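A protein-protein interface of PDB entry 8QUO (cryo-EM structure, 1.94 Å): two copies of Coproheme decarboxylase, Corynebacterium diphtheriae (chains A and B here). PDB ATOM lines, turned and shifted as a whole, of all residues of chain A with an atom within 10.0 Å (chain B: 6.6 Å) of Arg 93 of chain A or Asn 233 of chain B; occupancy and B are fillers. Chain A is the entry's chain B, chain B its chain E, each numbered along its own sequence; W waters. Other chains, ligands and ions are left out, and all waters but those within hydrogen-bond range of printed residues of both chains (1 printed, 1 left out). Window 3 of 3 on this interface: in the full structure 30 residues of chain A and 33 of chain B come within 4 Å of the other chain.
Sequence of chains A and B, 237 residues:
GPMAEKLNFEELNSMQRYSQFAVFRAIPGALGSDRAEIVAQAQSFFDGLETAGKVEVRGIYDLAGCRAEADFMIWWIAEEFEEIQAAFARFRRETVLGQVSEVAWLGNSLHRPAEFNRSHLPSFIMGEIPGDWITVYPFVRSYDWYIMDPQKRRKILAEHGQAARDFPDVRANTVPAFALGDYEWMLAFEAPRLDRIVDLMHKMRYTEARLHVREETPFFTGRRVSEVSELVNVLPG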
ATOM      1  N   PHE A  24      20.376  21.570  32.231  1.00  0.00           N
ATOM      2  CA  PHE A  24      20.496  22.637  31.255  1.00  0.00           C
ATOM      3  C   PHE A  24      21.893  23.242  31.289  1.00  0.00           C
ATOM      4  O   PHE A  24      22.522  23.349  32.349  1.00  0.00           O
ATOM      5  CB  PHE A  24      19.465  23.737  31.498  1.00  0.00           C
ATOM      6  CG  PHE A  24      18.047  23.293  31.311  1.00  0.00           C
ATOM      7  CD1 PHE A  24      17.325  22.777  32.370  1.00  0.00           C
ATOM      8  CD2 PHE A  24      17.434  23.396  30.076  1.00  0.00           C
ATOM      9  CE1 PHE A  24      16.019  22.372  32.201  1.00  0.00           C
ATOM     10  CE2 PHE A  24      16.128  22.991  29.902  1.00  0.00           C
ATOM     11  CZ  PHE A  24      15.421  22.477  30.966  1.00  0.00           C
ATOM     12  N   GLN A  41      10.500  36.697  35.921  1.00  0.00           N
ATOM     13  CA  GLN A  41       9.719  35.826  35.048  1.00  0.00           C
ATOM     14  C   GLN A  41       9.893  34.358  35.423  1.00  0.00           C
ATOM     15  O   GLN A  41       8.915  33.602  35.456  1.00  0.00           O
ATOM     16  CB  GLN A  41      10.111  36.063  33.591  1.00  0.00           C
ATOM     17  CG  GLN A  41       9.286  35.277  32.590  1.00  0.00           C
ATOM     18  CD  GLN A  41       9.828  35.387  31.182  1.00  0.00           C
ATOM     19  OE1 GLN A  41      10.994  35.089  30.930  1.00  0.00           O
ATOM     20  NE2 GLN A  41       8.983  35.820  30.255  1.00  0.00           N
ATOM     21  N   PHE A  45       7.036  31.818  36.798  1.00  0.00           N
ATOM     22  CA  PHE A  45       6.765  30.524  36.177  1.00  0.00           C
ATOM     23  C   PHE A  45       6.735  29.413  37.219  1.00  0.00           C
ATOM     24  O   PHE A  45       5.831  28.567  37.222  1.00  0.00           O
ATOM     25  CB  PHE A  45       7.813  30.228  35.103  1.00  0.00           C
ATOM     26  CG  PHE A  45       7.864  28.785  34.685  1.00  0.00           C
ATOM     27  CD1 PHE A  45       6.951  28.281  33.776  1.00  0.00           C
ATOM     28  CD2 PHE A  45       8.830  27.935  35.196  1.00  0.00           C
ATOM     29  CE1 PHE A  45       6.996  26.957  33.391  1.00  0.00           C
ATOM     30  CE2 PHE A  45       8.877  26.610  34.815  1.00  0.00           C
ATOM     31  CZ  PHE A  45       7.960  26.121  33.911  1.00  0.00           C
ATOM     32  N   TRP A  76      11.915  17.689  39.112  1.00  0.00           N
ATOM     33  CA  TRP A  76      10.485  17.839  39.347  1.00  0.00           C
ATOM     34  C   TRP A  76       9.753  16.523  39.123  1.00  0.00           C
ATOM     35  O   TRP A  76      10.174  15.677  38.331  1.00  0.00           O
ATOM     36  CB  TRP A  76       9.858  18.946  38.477  1.00  0.00           C
ATOM     37  CG  TRP A  76      10.180  18.900  37.016  1.00  0.00           C
ATOM     38  CD1 TRP A  76      10.520  17.807  36.277  1.00  0.00           C
ATOM     39  CD2 TRP A  76      10.164  20.007  36.108  1.00  0.00           C
ATOM     40  NE1 TRP A  76      10.733  18.167  34.970  1.00  0.00           N
ATOM     41  CE2 TRP A  76      10.519  19.514  34.840  1.00  0.00           C
ATOM     42  CE3 TRP A  76       9.889  21.370  36.248  1.00  0.00           C
ATOM     43  CZ2 TRP A  76      10.606  20.332  33.720  1.00  0.00           C
ATOM     44  CZ3 TRP A  76       9.978  22.181  35.134  1.00  0.00           C
ATOM     45  CH2 TRP A  76      10.333  21.661  33.887  1.00  0.00           C
ATOM     46  N   ILE A  84       4.665  16.557  33.141  1.00  0.00           N
ATOM     47  CA  ILE A  84       6.092  16.860  33.089  1.00  0.00           C
ATOM     48  C   ILE A  84       6.479  17.362  31.703  1.00  0.00           C
ATOM     49  O   ILE A  84       7.262  18.309  31.567  1.00  0.00           O
ATOM     50  CB  ILE A  84       6.919  15.628  33.501  1.00  0.00           C
ATOM     51  CG1 ILE A  84       6.881  15.448  35.019  1.00  0.00           C
ATOM     52  CG2 ILE A  84       8.355  15.755  33.025  1.00  0.00           C
ATOM     53  CD1 ILE A  84       7.589  14.208  35.501  1.00  0.00           C
ATOM     54  N   GLN A  85       5.940  16.735  30.654  1.00  0.00           N
ATOM     55  CA  GLN A  85       6.207  17.196  29.295  1.00  0.00           C
ATOM     56  C   GLN A  85       5.747  18.634  29.105  1.00  0.00           C
ATOM     57  O   GLN A  85       6.467  19.462  28.534  1.00  0.00           O
ATOM     58  CB  GLN A  85       5.507  16.285  28.287  1.00  0.00           C
ATOM     59  CG  GLN A  85       6.126  14.918  28.118  1.00  0.00           C
ATOM     60  CD  GLN A  85       5.622  14.214  26.876  1.00  0.00           C
ATOM     61  OE1 GLN A  85       4.441  13.884  26.776  1.00  0.00           O
ATOM     62  NE2 GLN A  85       6.511  13.987  25.920  1.00  0.00           N
ATOM     63  N   ALA A  86       4.538  18.946  29.576  1.00  0.00           N
ATOM     64  CA  ALA A  86       4.005  20.297  29.436  1.00  0.00           C
ATOM     65  C   ALA A  86       4.843  21.305  30.208  1.00  0.00           C
ATOM     66  O   ALA A  86       5.130  22.396  29.704  1.00  0.00           O
ATOM     67  CB  ALA A  86       2.551  20.337  29.902  1.00  0.00           C
ATOM     68  N   ALA A  87       5.245  20.959  31.433  1.00  0.00           N
ATOM     69  CA  ALA A  87       6.062  21.873  32.225  1.00  0.00           C
ATOM     70  C   ALA A  87       7.415  22.112  31.570  1.00  0.00           C
ATOM     71  O   ALA A  87       7.888  23.251  31.509  1.00  0.00           O
ATOM     72  CB  ALA A  87       6.239  21.326  33.641  1.00  0.00           C
ATOM     73  N   PHE A  88       8.047  21.051  31.065  1.00  0.00           N
ATOM     74  CA  PHE A  88       9.349  21.181  30.418  1.00  0.00           C
ATOM     75  C   PHE A  88       9.255  22.038  29.159  1.00  0.00           C
ATOM     76  O   PHE A  88      10.060  22.959  28.953  1.00  0.00           O
ATOM     77  CB  PHE A  88       9.886  19.782  30.105  1.00  0.00           C
ATOM     78  CG  PHE A  88      11.171  19.768  29.335  1.00  0.00           C
ATOM     79  CD1 PHE A  88      12.381  19.949  29.977  1.00  0.00           C
ATOM     80  CD2 PHE A  88      11.171  19.530  27.973  1.00  0.00           C
ATOM     81  CE1 PHE A  88      13.564  19.921  29.271  1.00  0.00           C
ATOM     82  CE2 PHE A  88      12.351  19.501  27.262  1.00  0.00           C
ATOM     83  CZ  PHE A  88      13.549  19.694  27.913  1.00  0.00           C
ATOM     84  N   ALA A  89       8.261  21.757  28.312  1.00  0.00           N
ATOM     85  CA  ALA A  89       8.079  22.542  27.098  1.00  0.00           C
ATOM     86  C   ALA A  89       7.759  23.994  27.423  1.00  0.00           C
ATOM     87  O   ALA A  89       8.270  24.909  26.769  1.00  0.00           O
ATOM     88  CB  ALA A  89       6.978  21.926  26.236  1.00  0.00           C
ATOM     89  N   ARG A  90       6.911  24.226  28.428  1.00  0.00           N
ATOM     90  CA  ARG A  90       6.566  25.594  28.801  1.00  0.00           C
ATOM     91  C   ARG A  90       7.777  26.341  29.345  1.00  0.00           C
ATOM     92  O   ARG A  90       7.948  27.534  29.070  1.00  0.00           O
ATOM     93  CB  ARG A  90       5.430  25.597  29.822  1.00  0.00           C
ATOM     94  CG  ARG A  90       4.816  26.970  30.046  1.00  0.00           C
ATOM     95  CD  ARG A  90       3.648  26.924  31.017  1.00  0.00           C
ATOM     96  NE  ARG A  90       3.106  25.580  31.171  1.00  0.00           N
ATOM     97  CZ  ARG A  90       2.101  25.090  30.458  1.00  0.00           C
ATOM     98  NH1 ARG A  90       1.501  25.810  29.524  1.00  0.00           N
ATOM     99  NH2 ARG A  90       1.688  23.847  30.687  1.00  0.00           N
ATOM    100  N   PHE A  91       8.622  25.664  30.125  1.00  0.00           N
ATOM    101  CA  PHE A  91       9.836  26.305  30.619  1.00  0.00           C
ATOM    102  C   PHE A  91      10.758  26.679  29.469  1.00  0.00           C
ATOM    103  O   PHE A  91      11.350  27.765  29.464  1.00  0.00           O
ATOM    104  CB  PHE A  91      10.559  25.391  31.606  1.00  0.00           C
ATOM    105  CG  PHE A  91      11.889  25.921  32.054  1.00  0.00           C
ATOM    106  CD1 PHE A  91      11.962  26.958  32.967  1.00  0.00           C
ATOM    107  CD2 PHE A  91      13.065  25.392  31.556  1.00  0.00           C
ATOM    108  CE1 PHE A  91      13.182  27.451  33.378  1.00  0.00           C
ATOM    109  CE2 PHE A  91      14.289  25.882  31.965  1.00  0.00           C
ATOM    110  CZ  PHE A  91      14.346  26.912  32.877  1.00  0.00           C
ATOM    111  N   ARG A  92      10.890  25.793  28.480  1.00  0.00           N
ATOM    112  CA  ARG A  92      11.734  26.111  27.334  1.00  0.00           C
ATOM    113  C   ARG A  92      11.127  27.174  26.427  1.00  0.00           C
ATOM    114  O   ARG A  92      11.869  27.859  25.716  1.00  0.00           O
ATOM    115  CB  ARG A  92      12.018  24.849  26.521  1.00  0.00           C
ATOM    116  CG  ARG A  92      12.966  23.887  27.197  1.00  0.00           C
ATOM    117  CD  ARG A  92      13.299  22.730  26.284  1.00  0.00           C
ATOM    118  NE  ARG A  92      14.201  23.118  25.208  1.00  0.00           N
ATOM    119  CZ  ARG A  92      14.296  22.482  24.049  1.00  0.00           C
ATOM    120  NH1 ARG A  92      13.554  21.420  23.781  1.00  0.00           N
ATOM    121  NH2 ARG A  92      15.159  22.919  23.138  1.00  0.00           N
ATOM    122  N   ARG A  93       9.805  27.331  26.433  1.00  0.00           N
ATOM    123  CA  ARG A  93       9.120  28.166  25.454  1.00  0.00           C
ATOM    124  C   ARG A  93       8.778  29.564  25.956  1.00  0.00           C
ATOM    125  O   ARG A  93       8.917  30.529  25.201  1.00  0.00           O
ATOM    126  CB  ARG A  93       7.837  27.464  24.995  1.00  0.00           C
ATOM    127  CG  ARG A  93       7.130  28.125  23.829  1.00  0.00           C
ATOM    128  CD  ARG A  93       5.895  27.337  23.425  1.00  0.00           C
ATOM    129  NE  ARG A  93       4.894  27.301  24.485  1.00  0.00           N
ATOM    130  CZ  ARG A  93       4.614  26.231  25.217  1.00  0.00           C
ATOM    131  NH1 ARG A  93       5.248  25.085  25.035  1.00  0.00           N
ATOM    132  NH2 ARG A  93       3.678  26.315  26.156  1.00  0.00           N
ATOM    133  N   GLU A  94       8.335  29.706  27.204  1.00  0.00           N
ATOM    134  CA  GLU A  94       7.741  30.948  27.678  1.00  0.00           C
ATOM    135  C   GLU A  94       8.594  31.677  28.710  1.00  0.00           C
ATOM    136  O   GLU A  94       8.147  32.687  29.261  1.00  0.00           O
ATOM    137  CB  GLU A  94       6.352  30.670  28.255  1.00  0.00           C
ATOM    138  CG  GLU A  94       5.475  29.822  27.353  1.00  0.00           C
ATOM    139  CD  GLU A  94       4.032  29.786  27.808  1.00  0.00           C
ATOM    140  OE1 GLU A  94       3.723  30.387  28.858  1.00  0.00           O
ATOM    141  OE2 GLU A  94       3.205  29.157  27.116  1.00  0.00           O
ATOM    142  N   THR A  95       9.801  31.196  28.991  1.00  0.00           N
ATOM    143  CA  THR A  95      10.706  31.863  29.916  1.00  0.00           C
ATOM    144  C   THR A  95      12.002  32.209  29.200  1.00  0.00           C
ATOM    145  O   THR A  95      12.507  31.420  28.397  1.00  0.00           O
ATOM    146  CB  THR A  95      11.011  30.993  31.142  1.00  0.00           C
ATOM    147  OG1 THR A  95      11.765  29.844  30.741  1.00  0.00           O
ATOM    148  CG2 THR A  95       9.726  30.543  31.812  1.00  0.00           C
ATOM    149  N   VAL A  96      12.530  33.401  29.489  1.00  0.00           N
ATOM    150  CA  VAL A  96      13.800  33.811  28.900  1.00  0.00           C
ATOM    151  C   VAL A  96      14.918  32.882  29.353  1.00  0.00           C
ATOM    152  O   VAL A  96      15.817  32.541  28.576  1.00  0.00           O
ATOM    153  CB  VAL A  96      14.102  35.280  29.248  1.00  0.00           C
ATOM    154  CG1 VAL A  96      15.493  35.668  28.777  1.00  0.00           C
ATOM    155  CG2 VAL A  96      13.059  36.193  28.631  1.00  0.00           C
ATOM    156  N   LEU A  97      14.871  32.445  30.615  1.00  0.00           N
ATOM    157  CA  LEU A  97      15.878  31.513  31.114  1.00  0.00           C
ATOM    158  C   LEU A  97      15.854  30.208  30.329  1.00  0.00           C
ATOM    159  O   LEU A  97      16.909  29.652  30.002  1.00  0.00           O
ATOM    160  CB  LEU A  97      15.653  31.250  32.603  1.00  0.00           C
ATOM    161  CG  LEU A  97      16.603  30.266  33.287  1.00  0.00           C
ATOM    162  CD1 LEU A  97      18.038  30.750  33.190  1.00  0.00           C
ATOM    163  CD2 LEU A  97      16.202  30.055  34.735  1.00  0.00           C
ATOM    164  N   GLY A  98      14.660  29.701  30.021  1.00  0.00           N
ATOM    165  CA  GLY A  98      14.560  28.516  29.188  1.00  0.00           C
ATOM    166  C   GLY A  98      15.016  28.743  27.761  1.00  0.00           C
ATOM    167  O   GLY A  98      15.580  27.841  27.137  1.00  0.00           O
ATOM    168  N   GLN A  99      14.778  29.942  27.223  1.00  0.00           N
ATOM    169  CA  GLN A  99      15.124  30.210  25.832  1.00  0.00           C
ATOM    170  C   GLN A  99      16.624  30.381  25.635  1.00  0.00           C
ATOM    171  O   GLN A  99      17.140  30.087  24.552  1.00  0.00           O
ATOM    172  CB  GLN A  99      14.384  31.454  25.338  1.00  0.00           C
ATOM    173  CG  GLN A  99      12.885  31.270  25.188  1.00  0.00           C
ATOM    174  CD  GLN A  99      12.126  32.576  25.309  1.00  0.00           C
ATOM    175  OE1 GLN A  99      12.716  33.653  25.272  1.00  0.00           O
ATOM    176  NE2 GLN A  99      10.812  32.484  25.457  1.00  0.00           N
ATOM    177  N   VAL A 100      17.339  30.851  26.653  1.00  0.00           N
ATOM    178  CA  VAL A 100      18.768  31.109  26.541  1.00  0.00           C
ATOM    179  C   VAL A 100      19.596  29.932  27.065  1.00  0.00           C
ATOM    180  O   VAL A 100      20.793  30.077  27.301  1.00  0.00           O
ATOM    181  CB  VAL A 100      19.161  32.419  27.240  1.00  0.00           C
ATOM    182  CG1 VAL A 100      18.323  33.571  26.714  1.00  0.00           C
ATOM    183  CG2 VAL A 100      19.012  32.288  28.747  1.00  0.00           C
ATOM    184  N   SER A 101      18.977  28.769  27.243  1.00  0.00           N
ATOM    185  CA  SER A 101      19.664  27.590  27.744  1.00  0.00           C
ATOM    186  C   SER A 101      19.427  26.416  26.807  1.00  0.00           C
ATOM    187  O   SER A 101      18.378  26.315  26.166  1.00  0.00           O
ATOM    188  CB  SER A 101      19.194  27.224  29.158  1.00  0.00           C
ATOM    189  OG  SER A 101      19.395  28.300  30.055  1.00  0.00           O
ATOM    190  N   VAL A 103      19.294  22.148  26.372  1.00  0.00           N
ATOM    191  CA  VAL A 103      19.044  20.929  27.132  1.00  0.00           C
ATOM    192  C   VAL A 103      20.242  20.006  26.959  1.00  0.00           C
ATOM    193  O   VAL A 103      20.545  19.573  25.842  1.00  0.00           O
ATOM    194  CB  VAL A 103      17.747  20.247  26.679  1.00  0.00           C
ATOM    195  CG1 VAL A 103      17.469  19.025  27.534  1.00  0.00           C
ATOM    196  CG2 VAL A 103      16.591  21.223  26.746  1.00  0.00           C
ATOM    197  N   LEU B  31      11.591  29.053  15.222  1.00  0.00           N
ATOM    198  CA  LEU B  31      10.169  28.915  14.931  1.00  0.00           C
ATOM    199  C   LEU B  31       9.420  30.229  15.116  1.00  0.00           C
ATOM    200  O   LEU B  31       8.496  30.530  14.353  1.00  0.00           O
ATOM    201  CB  LEU B  31       9.559  27.825  15.812  1.00  0.00           C
ATOM    202  CG  LEU B  31       8.172  27.323  15.412  1.00  0.00           C
ATOM    203  CD1 LEU B  31       8.154  26.904  13.954  1.00  0.00           C
ATOM    204  CD2 LEU B  31       7.748  26.171  16.304  1.00  0.00           C
ATOM    205  N   ARG B  35       2.599  31.299  14.795  1.00  0.00           N
ATOM    206  CA  ARG B  35       2.701  29.964  14.220  1.00  0.00           C
ATOM    207  C   ARG B  35       1.435  29.513  13.502  1.00  0.00           C
ATOM    208  O   ARG B  35       1.330  28.332  13.152  1.00  0.00           O
ATOM    209  CB  ARG B  35       3.061  28.948  15.309  1.00  0.00           C
ATOM    210  CG  ARG B  35       4.286  29.321  16.120  1.00  0.00           C
ATOM    211  CD  ARG B  35       4.579  28.285  17.186  1.00  0.00           C
ATOM    212  NE  ARG B  35       5.667  28.703  18.061  1.00  0.00           N
ATOM    213  CZ  ARG B  35       6.200  27.944  19.007  1.00  0.00           C
ATOM    214  NH1 ARG B  35       5.771  26.715  19.231  1.00  0.00           N
ATOM    215  NH2 ARG B  35       7.190  28.432  19.747  1.00  0.00           N
ATOM    216  N   ALA B  36       0.473  30.407  13.272  1.00  0.00           N
ATOM    217  CA  ALA B  36      -0.759  30.007  12.600  1.00  0.00           C
ATOM    218  C   ALA B  36      -0.492  29.578  11.162  1.00  0.00           C
ATOM    219  O   ALA B  36      -0.976  28.531  10.713  1.00  0.00           O
ATOM    220  CB  ALA B  36      -1.776  31.147  12.643  1.00  0.00           C
ATOM    221  N   VAL B  39       1.410  26.287  11.069  1.00  0.00           N
ATOM    222  CA  VAL B  39       0.496  25.180  11.334  1.00  0.00           C
ATOM    223  C   VAL B  39      -0.331  24.865  10.096  1.00  0.00           C
ATOM    224  O   VAL B  39      -0.505  23.697   9.728  1.00  0.00           O
ATOM    225  CB  VAL B  39      -0.400  25.509  12.542  1.00  0.00           C
ATOM    226  CG1 VAL B  39      -1.682  24.697  12.494  1.00  0.00           C
ATOM    227  CG2 VAL B  39       0.343  25.258  13.838  1.00  0.00           C
ATOM    228  N   VAL B 228      -1.191  18.210  13.814  1.00  0.00           N
ATOM    229  CA  VAL B 228       0.123  18.838  13.844  1.00  0.00           C
ATOM    230  C   VAL B 228       0.109  20.171  14.583  1.00  0.00           C
ATOM    231  O   VAL B 228       1.161  20.626  15.046  1.00  0.00           O
ATOM    232  CB  VAL B 228       0.663  19.004  12.410  1.00  0.00           C
ATOM    233  CG1 VAL B 228       0.055  20.225  11.739  1.00  0.00           C
ATOM    234  CG2 VAL B 228       2.183  19.087  12.417  1.00  0.00           C
ATOM    235  N   SER B 229      -1.055  20.814  14.712  1.00  0.00           N
ATOM    236  CA  SER B 229      -1.126  22.069  15.452  1.00  0.00           C
ATOM    237  C   SER B 229      -0.765  21.866  16.917  1.00  0.00           C
ATOM    238  O   SER B 229      -0.070  22.695  17.517  1.00  0.00           O
ATOM    239  CB  SER B 229      -2.522  22.675  15.328  1.00  0.00           C
ATOM    240  OG  SER B 229      -3.463  21.947  16.094  1.00  0.00           O
ATOM    241  N   GLU B 230      -1.238  20.766  17.508  1.00  0.00           N
ATOM    242  CA  GLU B 230      -0.923  20.466  18.899  1.00  0.00           C
ATOM    243  C   GLU B 230       0.578  20.311  19.101  1.00  0.00           C
ATOM    244  O   GLU B 230       1.121  20.720  20.133  1.00  0.00           O
ATOM    245  CB  GLU B 230      -1.661  19.200  19.331  1.00  0.00           C
ATOM    246  CG  GLU B 230      -1.414  18.780  20.766  1.00  0.00           C
ATOM    247  CD  GLU B 230      -2.209  17.547  21.151  1.00  0.00           C
ATOM    248  OE1 GLU B 230      -3.084  17.133  20.364  1.00  0.00           O
ATOM    249  OE2 GLU B 230      -1.958  16.992  22.242  1.00  0.00           O
ATOM    250  N   LEU B 231       1.266  19.719  18.124  1.00  0.00           N
ATOM    251  CA  LEU B 231       2.714  19.580  18.224  1.00  0.00           C
ATOM    252  C   LEU B 231       3.418  20.916  18.027  1.00  0.00           C
ATOM    253  O   LEU B 231       4.345  21.251  18.774  1.00  0.00           O
ATOM    254  CB  LEU B 231       3.214  18.563  17.203  1.00  0.00           C
ATOM    255  CG  LEU B 231       4.733  18.542  17.060  1.00  0.00           C
ATOM    256  CD1 LEU B 231       5.351  17.951  18.313  1.00  0.00           C
ATOM    257  CD2 LEU B 231       5.154  17.773  15.823  1.00  0.00           C
ATOM    258  N   VAL B 232       2.996  21.693  17.028  1.00  0.00           N
ATOM    259  CA  VAL B 232       3.694  22.934  16.708  1.00  0.00           C
ATOM    260  C   VAL B 232       3.546  23.945  17.838  1.00  0.00           C
ATOM    261  O   VAL B 232       4.480  24.697  18.140  1.00  0.00           O
ATOM    262  CB  VAL B 232       3.192  23.497  15.366  1.00  0.00           C
ATOM    263  CG1 VAL B 232       3.746  24.891  15.125  1.00  0.00           C
ATOM    264  CG2 VAL B 232       3.583  22.573  14.227  1.00  0.00           C
ATOM    265  N   ASN B 233       2.384  23.971  18.493  1.00  0.00           N
ATOM    266  CA  ASN B 233       2.144  24.977  19.521  1.00  0.00           C
ATOM    267  C   ASN B 233       2.966  24.762  20.786  1.00  0.00           C
ATOM    268  O   ASN B 233       3.005  25.662  21.631  1.00  0.00           O
ATOM    269  CB  ASN B 233       0.657  25.017  19.872  1.00  0.00           C
ATOM    270  CG  ASN B 233      -0.170  25.721  18.815  1.00  0.00           C
ATOM    271  OD1 ASN B 233       0.331  26.578  18.090  1.00  0.00           O
ATOM    272  ND2 ASN B 233      -1.442  25.359  18.722  1.00  0.00           N
ATOM    273  N   VAL B 234       3.620  23.612  20.945  1.00  0.00           N
ATOM    274  CA  VAL B 234       4.423  23.342  22.134  1.00  0.00           C
ATOM    275  C   VAL B 234       5.919  23.369  21.862  1.00  0.00           C
ATOM    276  O   VAL B 234       6.704  23.281  22.820  1.00  0.00           O
ATOM    277  CB  VAL B 234       4.036  21.999  22.787  1.00  0.00           C
ATOM    278  CG1 VAL B 234       2.532  21.910  22.969  1.00  0.00           C
ATOM    279  CG2 VAL B 234       4.553  20.833  21.963  1.00  0.00           C
ATOM    280  N   LEU B 235       6.341  23.484  20.607  1.00  0.00           N
ATOM    281  CA  LEU B 235       7.759  23.487  20.294  1.00  0.00           C
ATOM    282  C   LEU B 235       8.420  24.768  20.804  1.00  0.00           C
ATOM    283  O   LEU B 235       7.771  25.811  20.908  1.00  0.00           O
ATOM    284  CB  LEU B 235       7.973  23.355  18.790  1.00  0.00           C
ATOM    285  CG  LEU B 235       7.673  21.986  18.182  1.00  0.00           C
ATOM    286  CD1 LEU B 235       7.733  22.051  16.667  1.00  0.00           C
ATOM    287  CD2 LEU B 235       8.636  20.942  18.717  1.00  0.00           C
ATOM    288  N   PRO B 236       9.709  24.710  21.140  1.00  0.00           N
ATOM    289  CA  PRO B 236      10.410  25.924  21.571  1.00  0.00           C
ATOM    290  C   PRO B 236      10.448  26.967  20.465  1.00  0.00           C
ATOM    291  O   PRO B 236      10.546  26.644  19.279  1.00  0.00           O
ATOM    292  CB  PRO B 236      11.818  25.423  21.916  1.00  0.00           C
ATOM    293  CG  PRO B 236      11.677  23.953  22.096  1.00  0.00           C
ATOM    294  CD  PRO B 236      10.579  23.524  21.185  1.00  0.00           C
ATOM    295  N   GLY B 237      10.373  28.230  20.868  1.00  0.00           N
ATOM    296  CA  GLY B 237      10.351  29.337  19.931  1.00  0.00           C
ATOM    297  C   GLY B 237      11.604  29.465  19.090  1.00  0.00           C
ATOM    298  O   GLY B 237      12.625  28.843  19.376  1.00  0.00           O
ATOM    299  OXT GLY B 237      11.632  30.196  18.099  1.00  0.00           O
HETATM  300  O   HOH W   1       8.879  24.088  24.158  1.00  0.00           O
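The backbone carbonyl oxygen (O) of Val 234 of chain B lies within hydrogen-bond range of the guanidinium group (NH1) of Arg 93 of chain A, 3.2 Å away.
The backbone carbonyl oxygen (O) of Leu 235 of chain B sits at hydrogen-bond distance from the guanidinium group (NH1) of Arg 35 of chain B (2.8 Å).
The side-chain amide nitrogen of Asn 233 of chain B lies within hydrogen-bond range of the backbone carbonyl oxygen of Ser 229 of chain B.
The guanidinium group (NH2) of Arg 93 of chain A lies within salt-bridge range of the side-chain carboxylate (OE2) of Glu 94 of chain A.
The guanidinium group of Arg 93 of chain A lies close to the backbone carbonyl oxygen of Ala 89 of chain A, at 3.5 Å.
The side-chain amide nitrogen (NE2) of Gln 99 of chain A is in hydrogen-bond range of the backbone carbonyl oxygen (O) of Arg 93 of chain A, 2.7 Å away.
Among the printed residues, merely in contact across the chains: Arg 93 of chain A with Leu 235 of chain B (3.5 Å), Arg 92 of chain A with Pro 236 of chain B (3.6 Å), Ala 89 of chain A with Val 234 of chain B (3.7 Å) and Arg 93 of chain A with Asn 233 of chain B (3.8 Å).
Printed residues of chain B within 4 Å of Ala 89 of chain A: Val 234.
Of the printed residues of chain B, Arg 92 of chain A touches Pro 236.
No residue of chain A comes within 4 Å of Val 232 of chain B.
Of the printed residues of chain A, Asn 233 of chain B touches Arg 93.
Of the printed residues of chain A, Val 234 of chain B touches Ala 89 (3.7 Å) and Arg 93 (3.2 Å).
Of the printed residues of chain A, Leu 235 of chain B touches Arg 93.
Of the printed residues of chain A, Pro 236 of chain B touches Arg 92.
The nearest residue of chain B that does not touch Arg 93 of chain A is Arg 35 of chain B (4.1 Å).
The nearest residue of chain A that does not touch Asn 233 of chain B is Glu 94 of chain A (6.5 Å).
Of the 23 printed residues of chain A, 3 touch a printed residue of chain B.
Hydrophobic or aromatic side chains of chain A within 4 Å of the printed part of chain B: Ala 89.
No position is printed for both chains.
Of the 5 pairs that touch across the chains among the printed residues, none has its exchanged pair printed and touching as well.
Water W1 bridges O of Val 234 of chain B (2.7 Å) and O of Ala 89 of chain A (2.8 Å).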
